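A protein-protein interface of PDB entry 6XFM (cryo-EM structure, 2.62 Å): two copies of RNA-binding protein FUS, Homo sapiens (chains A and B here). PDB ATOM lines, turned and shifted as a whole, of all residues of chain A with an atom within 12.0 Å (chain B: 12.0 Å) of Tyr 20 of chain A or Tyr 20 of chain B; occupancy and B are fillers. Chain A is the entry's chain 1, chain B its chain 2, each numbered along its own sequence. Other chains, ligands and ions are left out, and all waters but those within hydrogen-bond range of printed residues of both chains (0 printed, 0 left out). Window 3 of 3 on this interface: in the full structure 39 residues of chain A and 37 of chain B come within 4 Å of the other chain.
The side-chain amide nitrogen (NE2) of Gln 22 of chain A is in hydrogen-bond range of the side-chain amide oxygen (OE1) of Gln 22 of chain B.
NE2 of Gln 23 of chain B sits at hydrogen-bond distance from O of Gln 16 of chain A, 3.3 Å away.
The backbone carbonyl oxygen of Gln 16 of chain A sits at hydrogen-bond distance from the backbone NH of Ser 17 of chain B (3.1 Å).
N of Gln 23 of chain A sits at hydrogen-bond distance from O of Gln 22 of chain B (2.8 Å).
The backbone NH of Tyr 20 of chain A is in hydrogen-bond range of the backbone carbonyl oxygen of Tyr 20 of chain B (2.8 Å).
OE1 of Gln 23 of chain A sits at hydrogen-bond distance from NE2 of Gln 23 of chain B, at 3.1 Å.
The backbone carbonyl oxygen of Gln 16 of chain A is in hydrogen-bond range of the backbone NH of Gly 18 of chain B, 3.1 Å away.
The backbone carbonyl oxygen (O) of Ser 19 of chain B is in hydrogen-bond range of the backbone NH (N) of Tyr 20 of chain A (3.3 Å).
O of Ser 21 of chain A lies within hydrogen-bond range of N of Gln 22 of chain B (3.2 Å).
NE2 of Gln 23 of chain B sits at hydrogen-bond distance from OG of Ser 21 of chain B (3.2 Å).
OG of Ser 21 of chain A lies within hydrogen-bond range of NE2 of Gln 23 of chain A (3.2 Å).
NE2 of Gln 23 of chain B sits close to N of Gly 18 of chain B (3.2 Å).
The side-chain amide nitrogen of Gln 16 of chain A is in hydrogen-bond range of the backbone carbonyl oxygen of Gln 23 of chain A.
NE2 of Gln 16 of chain B sits at hydrogen-bond distance from O of Gln 23 of chain B (2.7 Å).
NE2 of Gln 23 of chain A lies close to N of Gly 18 of chain A, 3.2 Å away.
Gln 16 of chain A touches Gln 16 of chain B.
Gln 16 of chain A touches Pro 24 of chain B.
Ser 17 of chain B touches Ser 17 of chain A.
Gly 18 of chain B touches Ser 17 of chain A.
O of Gly 18 of chain A touches CA of Gly 18 of chain B, at 3.3 Å.
Gly 18 of chain A touches Ser 21 of chain B.
Gly 18 of chain A touches Gln 23 of chain B.
Ser 19 of chain B touches Ser 19 of chain A (O to CA, 3.3 Å).
Ser 21 of chain A touches Ser 21 of chain B (O to CB, 3.1 Å).
Pro 24 of chain A touches Pro 24 of chain B.
Of the printed residues of chain B, Gly 18 of chain A touches Gly 18 (3.3 Å), Ser 19 (3.8 Å), Ser 21 (3.99 Å) and Gln 23 (3.9 Å).
Of the printed residues of chain B, Tyr 20 of chain A touches Ser 19, Tyr 20 and Ser 21.
Of chain B, only Tyr 20 (3.9 Å), Ser 21 (3.1 Å) and Gln 22 (3.2 Å) come within 4 Å of Ser 21 of chain A.
Printed residues of chain B within 4 Å of Gln 23 of chain A: Gln 22 (2.8 Å) and Gln 23 (3.1 Å).
Printed residues of chain A within 4 Å of Gln 16 of chain B: Gln 16.
Gly 18 of chain B touches three residues of chain A.
Ser 19 of chain B touches just these residues of chain A: Gly 18 (3.8 Å), Ser 19 (3.3 Å) and Tyr 20 (3.3 Å).
Tyr 20 of chain B touches just these residues of chain A: Tyr 20 and Ser 21.
Of the printed residues of chain A, Ser 21 of chain B touches Gly 18, Tyr 20 and Ser 21.
Of the printed residues of chain A, Gln 23 of chain B touches Gln 16 (3.3 Å), Gly 18 (3.9 Å) and Gln 23 (3.1 Å).
The nearest residue of chain B that does not touch Tyr 20 of chain A is Gln 22 of chain B (6.4 Å).
The nearest residue of chain A that does not touch Tyr 20 of chain B is Ser 19 of chain A (4.1 Å).
The nearest printed residue of chain A that does not touch Gln 23 of chain B is Ser 17 of chain A (4.7 Å).
Of the 9 printed residues of chain A, 9 touch a printed residue of chain B.
Hydrophobic or aromatic side chains of chain B within 4 Å of the printed part of chain A: Tyr 20 and Pro 24.
Among the printed residues, 22 pairs touch across the chains.
Gln 16 of chain A touches Ser 17 of chain B, but with the chains exchanged Ser 17 of chain A does not touch Gln 16 of chain B (5.8 Å).
Tyr 20 of chain A touches Ser 19 of chain B, but with the chains exchanged Ser 19 of chain A does not touch Tyr 20 of chain B (4.1 Å).
Tyr 20 of chain A touches its own counterpart, Tyr 20 of chain B.
Gln 23 of chain A touches its own counterpart, Gln 23 of chain B.
Of the 22 pairs that touch across the chains among the printed residues, 11 have their exchanged pair printed and touching as well.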
ATOM      1  N   GLN A  16      27.325 -11.596  21.574  1.00  0.00           N
ATOM      2  CA  GLN A  16      26.846 -12.774  20.842  1.00  0.00           C
ATOM      3  C   GLN A  16      27.253 -12.778  19.365  1.00  0.00           C
ATOM      4  O   GLN A  16      26.392 -12.699  18.479  1.00  0.00           O
ATOM      5  CB  GLN A  16      25.321 -12.852  20.937  1.00  0.00           C
ATOM      6  CG  GLN A  16      24.908 -13.178  22.373  1.00  0.00           C
ATOM      7  CD  GLN A  16      23.395 -13.054  22.517  1.00  0.00           C
ATOM      8  OE1 GLN A  16      22.765 -12.277  21.798  1.00  0.00           O
ATOM      9  NE2 GLN A  16      22.770 -13.778  23.406  1.00  0.00           N
ATOM     10  N   SER A  17      28.553 -12.886  19.094  1.00  0.00           N
ATOM     11  CA  SER A  17      29.027 -12.913  17.708  1.00  0.00           C
ATOM     12  C   SER A  17      29.704 -14.247  17.355  1.00  0.00           C
ATOM     13  O   SER A  17      30.127 -14.445  16.215  1.00  0.00           O
ATOM     14  CB  SER A  17      29.994 -11.757  17.463  1.00  0.00           C
ATOM     15  OG  SER A  17      31.125 -11.900  18.311  1.00  0.00           O
ATOM     16  N   GLY A  18      29.799 -15.163  18.321  1.00  0.00           N
ATOM     17  CA  GLY A  18      30.422 -16.466  18.070  1.00  0.00           C
ATOM     18  C   GLY A  18      29.535 -17.331  17.175  1.00  0.00           C
ATOM     19  O   GLY A  18      28.367 -17.013  16.955  1.00  0.00           O
ATOM     20  N   SER A  19      30.102 -18.413  16.646  1.00  0.00           N
ATOM     21  CA  SER A  19      29.348 -19.298  15.756  1.00  0.00           C
ATOM     22  C   SER A  19      29.354 -20.741  16.255  1.00  0.00           C
ATOM     23  O   SER A  19      30.298 -21.172  16.918  1.00  0.00           O
ATOM     24  CB  SER A  19      29.953 -19.255  14.356  1.00  0.00           C
ATOM     25  OG  SER A  19      29.855 -17.934  13.841  1.00  0.00           O
ATOM     26  N   TYR A  20      28.299 -21.486  15.918  1.00  0.00           N
ATOM     27  CA  TYR A  20      28.203 -22.889  16.327  1.00  0.00           C
ATOM     28  C   TYR A  20      28.337 -23.030  17.837  1.00  0.00           C
ATOM     29  O   TYR A  20      29.246 -23.707  18.317  1.00  0.00           O
ATOM     30  CB  TYR A  20      29.306 -23.711  15.660  1.00  0.00           C
ATOM     31  CG  TYR A  20      29.182 -23.637  14.156  1.00  0.00           C
ATOM     32  CD1 TYR A  20      29.958 -22.721  13.438  1.00  0.00           C
ATOM     33  CD2 TYR A  20      28.302 -24.492  13.477  1.00  0.00           C
ATOM     34  CE1 TYR A  20      29.856 -22.658  12.044  1.00  0.00           C
ATOM     35  CE2 TYR A  20      28.198 -24.428  12.082  1.00  0.00           C
ATOM     36  CZ  TYR A  20      28.977 -23.512  11.365  1.00  0.00           C
ATOM     37  OH  TYR A  20      28.880 -23.448   9.989  1.00  0.00           O
ATOM     38  N   SER A  21      27.450 -22.381  18.587  1.00  0.00           N
ATOM     39  CA  SER A  21      27.522 -22.450  20.045  1.00  0.00           C
ATOM     40  C   SER A  21      26.220 -22.007  20.712  1.00  0.00           C
ATOM     41  O   SER A  21      25.343 -21.440  20.077  1.00  0.00           O
ATOM     42  CB  SER A  21      28.663 -21.554  20.513  1.00  0.00           C
ATOM     43  OG  SER A  21      28.381 -20.216  20.134  1.00  0.00           O
ATOM     44  N   GLN A  22      26.116 -22.238  22.016  1.00  0.00           N
ATOM     45  CA  GLN A  22      24.935 -21.806  22.747  1.00  0.00           C
ATOM     46  C   GLN A  22      25.257 -20.487  23.429  1.00  0.00           C
ATOM     47  O   GLN A  22      26.151 -20.423  24.274  1.00  0.00           O
ATOM     48  CB  GLN A  22      24.518 -22.840  23.796  1.00  0.00           C
ATOM     49  CG  GLN A  22      23.890 -24.061  23.124  1.00  0.00           C
ATOM     50  CD  GLN A  22      23.466 -25.064  24.191  1.00  0.00           C
ATOM     51  OE1 GLN A  22      24.263 -25.429  25.055  1.00  0.00           O
ATOM     52  NE2 GLN A  22      22.247 -25.530  24.189  1.00  0.00           N
ATOM     53  N   GLN A  23      24.558 -19.429  23.039  1.00  0.00           N
ATOM     54  CA  GLN A  23      24.826 -18.121  23.606  1.00  0.00           C
ATOM     55  C   GLN A  23      23.553 -17.457  24.112  1.00  0.00           C
ATOM     56  O   GLN A  23      23.166 -16.391  23.632  1.00  0.00           O
ATOM     57  CB  GLN A  23      25.470 -17.235  22.538  1.00  0.00           C
ATOM     58  CG  GLN A  23      26.763 -17.885  22.047  1.00  0.00           C
ATOM     59  CD  GLN A  23      27.294 -17.116  20.845  1.00  0.00           C
ATOM     60  OE1 GLN A  23      26.516 -16.535  20.092  1.00  0.00           O
ATOM     61  NE2 GLN A  23      28.579 -17.075  20.619  1.00  0.00           N
ATOM     62  N   PRO A  24      22.923 -18.036  25.090  1.00  0.00           N
ATOM     63  CA  PRO A  24      21.700 -17.448  25.692  1.00  0.00           C
ATOM     64  C   PRO A  24      22.060 -16.223  26.533  1.00  0.00           C
ATOM     65  O   PRO A  24      23.132 -16.179  27.133  1.00  0.00           O
ATOM     66  CB  PRO A  24      21.144 -18.590  26.544  1.00  0.00           C
ATOM     67  CG  PRO A  24      22.328 -19.433  26.893  1.00  0.00           C
ATOM     68  CD  PRO A  24      23.296 -19.318  25.717  1.00  0.00           C
ATOM     69  N   GLN B  16      23.501 -10.057  18.811  1.00  0.00           N
ATOM     70  CA  GLN B  16      23.048 -11.218  18.035  1.00  0.00           C
ATOM     71  C   GLN B  16      23.469 -11.160  16.562  1.00  0.00           C
ATOM     72  O   GLN B  16      22.618 -11.063  15.673  1.00  0.00           O
ATOM     73  CB  GLN B  16      21.524 -11.323  18.109  1.00  0.00           C
ATOM     74  CG  GLN B  16      21.102 -11.708  19.529  1.00  0.00           C
ATOM     75  CD  GLN B  16      19.585 -11.613  19.658  1.00  0.00           C
ATOM     76  OE1 GLN B  16      18.950 -10.823  18.959  1.00  0.00           O
ATOM     77  NE2 GLN B  16      18.964 -12.373  20.516  1.00  0.00           N
ATOM     78  N   SER B  17      24.774 -11.237  16.301  1.00  0.00           N
ATOM     79  CA  SER B  17      25.261 -11.207  14.921  1.00  0.00           C
ATOM     80  C   SER B  17      25.963 -12.517  14.528  1.00  0.00           C
ATOM     81  O   SER B  17      26.394 -12.671  13.386  1.00  0.00           O
ATOM     82  CB  SER B  17      26.211 -10.028  14.726  1.00  0.00           C
ATOM     83  OG  SER B  17      27.338 -10.183  15.574  1.00  0.00           O
ATOM     84  N   GLY B  18      26.067 -13.464  15.464  1.00  0.00           N
ATOM     85  CA  GLY B  18      26.713 -14.749  15.171  1.00  0.00           C
ATOM     86  C   GLY B  18      25.847 -15.595  14.236  1.00  0.00           C
ATOM     87  O   GLY B  18      24.676 -15.287  14.015  1.00  0.00           O
ATOM     88  N   SER B  19      26.435 -16.651  13.675  1.00  0.00           N
ATOM     89  CA  SER B  19      25.704 -17.518  12.747  1.00  0.00           C
ATOM     90  C   SER B  19      25.726 -18.982  13.195  1.00  0.00           C
ATOM     91  O   SER B  19      26.668 -19.432  13.854  1.00  0.00           O
ATOM     92  CB  SER B  19      26.321 -17.411  11.352  1.00  0.00           C
ATOM     93  OG  SER B  19      26.201 -16.075  10.880  1.00  0.00           O
ATOM     94  N   TYR B  20      24.682 -19.725  12.818  1.00  0.00           N
ATOM     95  CA  TYR B  20      24.598 -21.143  13.171  1.00  0.00           C
ATOM     96  C   TYR B  20      24.714 -21.335  14.675  1.00  0.00           C
ATOM     97  O   TYR B  20      25.618 -22.019  15.138  1.00  0.00           O
ATOM     98  CB  TYR B  20      25.723 -21.922  12.489  1.00  0.00           C
ATOM     99  CG  TYR B  20      25.615 -21.795  10.986  1.00  0.00           C
ATOM    100  CD1 TYR B  20      26.385 -20.843  10.308  1.00  0.00           C
ATOM    101  CD2 TYR B  20      24.757 -22.638  10.270  1.00  0.00           C
ATOM    102  CE1 TYR B  20      26.295 -20.732   8.916  1.00  0.00           C
ATOM    103  CE2 TYR B  20      24.665 -22.527   8.876  1.00  0.00           C
ATOM    104  CZ  TYR B  20      25.436 -21.574   8.200  1.00  0.00           C
ATOM    105  OH  TYR B  20      25.350 -21.466   6.826  1.00  0.00           O
ATOM    106  N   SER B  21      23.818 -20.717  15.438  1.00  0.00           N
ATOM    107  CA  SER B  21      23.883 -20.835  16.892  1.00  0.00           C
ATOM    108  C   SER B  21      22.569 -20.440  17.564  1.00  0.00           C
ATOM    109  O   SER B  21      21.690 -19.862  16.944  1.00  0.00           O
ATOM    110  CB  SER B  21      25.001 -19.928  17.395  1.00  0.00           C
ATOM    111  OG  SER B  21      24.699 -18.590  17.044  1.00  0.00           O
ATOM    112  N   GLN B  22      22.458 -20.722  18.858  1.00  0.00           N
ATOM    113  CA  GLN B  22      21.264 -20.337  19.594  1.00  0.00           C
ATOM    114  C   GLN B  22      21.559 -19.039  20.327  1.00  0.00           C
ATOM    115  O   GLN B  22      22.442 -18.990  21.183  1.00  0.00           O
ATOM    116  CB  GLN B  22      20.853 -21.413  20.601  1.00  0.00           C
ATOM    117  CG  GLN B  22      20.252 -22.620  19.881  1.00  0.00           C
ATOM    118  CD  GLN B  22      19.830 -23.666  20.911  1.00  0.00           C
ATOM    119  OE1 GLN B  22      20.621 -24.043  21.772  1.00  0.00           O
ATOM    120  NE2 GLN B  22      18.620 -24.149  20.876  1.00  0.00           N
ATOM    121  N   GLN B  23      20.845 -17.980  19.966  1.00  0.00           N
ATOM    122  CA  GLN B  23      21.084 -16.688  20.582  1.00  0.00           C
ATOM    123  C   GLN B  23      19.798 -16.061  21.100  1.00  0.00           C
ATOM    124  O   GLN B  23      19.398 -14.986  20.656  1.00  0.00           O
ATOM    125  CB  GLN B  23      21.725 -15.754  19.554  1.00  0.00           C
ATOM    126  CG  GLN B  23      23.036 -16.365  19.056  1.00  0.00           C
ATOM    127  CD  GLN B  23      23.565 -15.546  17.887  1.00  0.00           C
ATOM    128  OE1 GLN B  23      22.784 -14.956  17.143  1.00  0.00           O
ATOM    129  NE2 GLN B  23      24.851 -15.475  17.679  1.00  0.00           N
ATOM    130  N   PRO B  24      19.164 -16.689  22.046  1.00  0.00           N
ATOM    131  CA  PRO B  24      17.930 -16.139  22.666  1.00  0.00           C
ATOM    132  C   PRO B  24      18.261 -14.943  23.553  1.00  0.00           C
ATOM    133  O   PRO B  24      19.326 -14.906  24.171  1.00  0.00           O
ATOM    134  CB  PRO B  24      17.382 -17.320  23.467  1.00  0.00           C
ATOM    135  CG  PRO B  24      18.576 -18.156  23.797  1.00  0.00           C
ATOM    136  CD  PRO B  24      19.554 -17.983  22.635  1.00  0.00           C
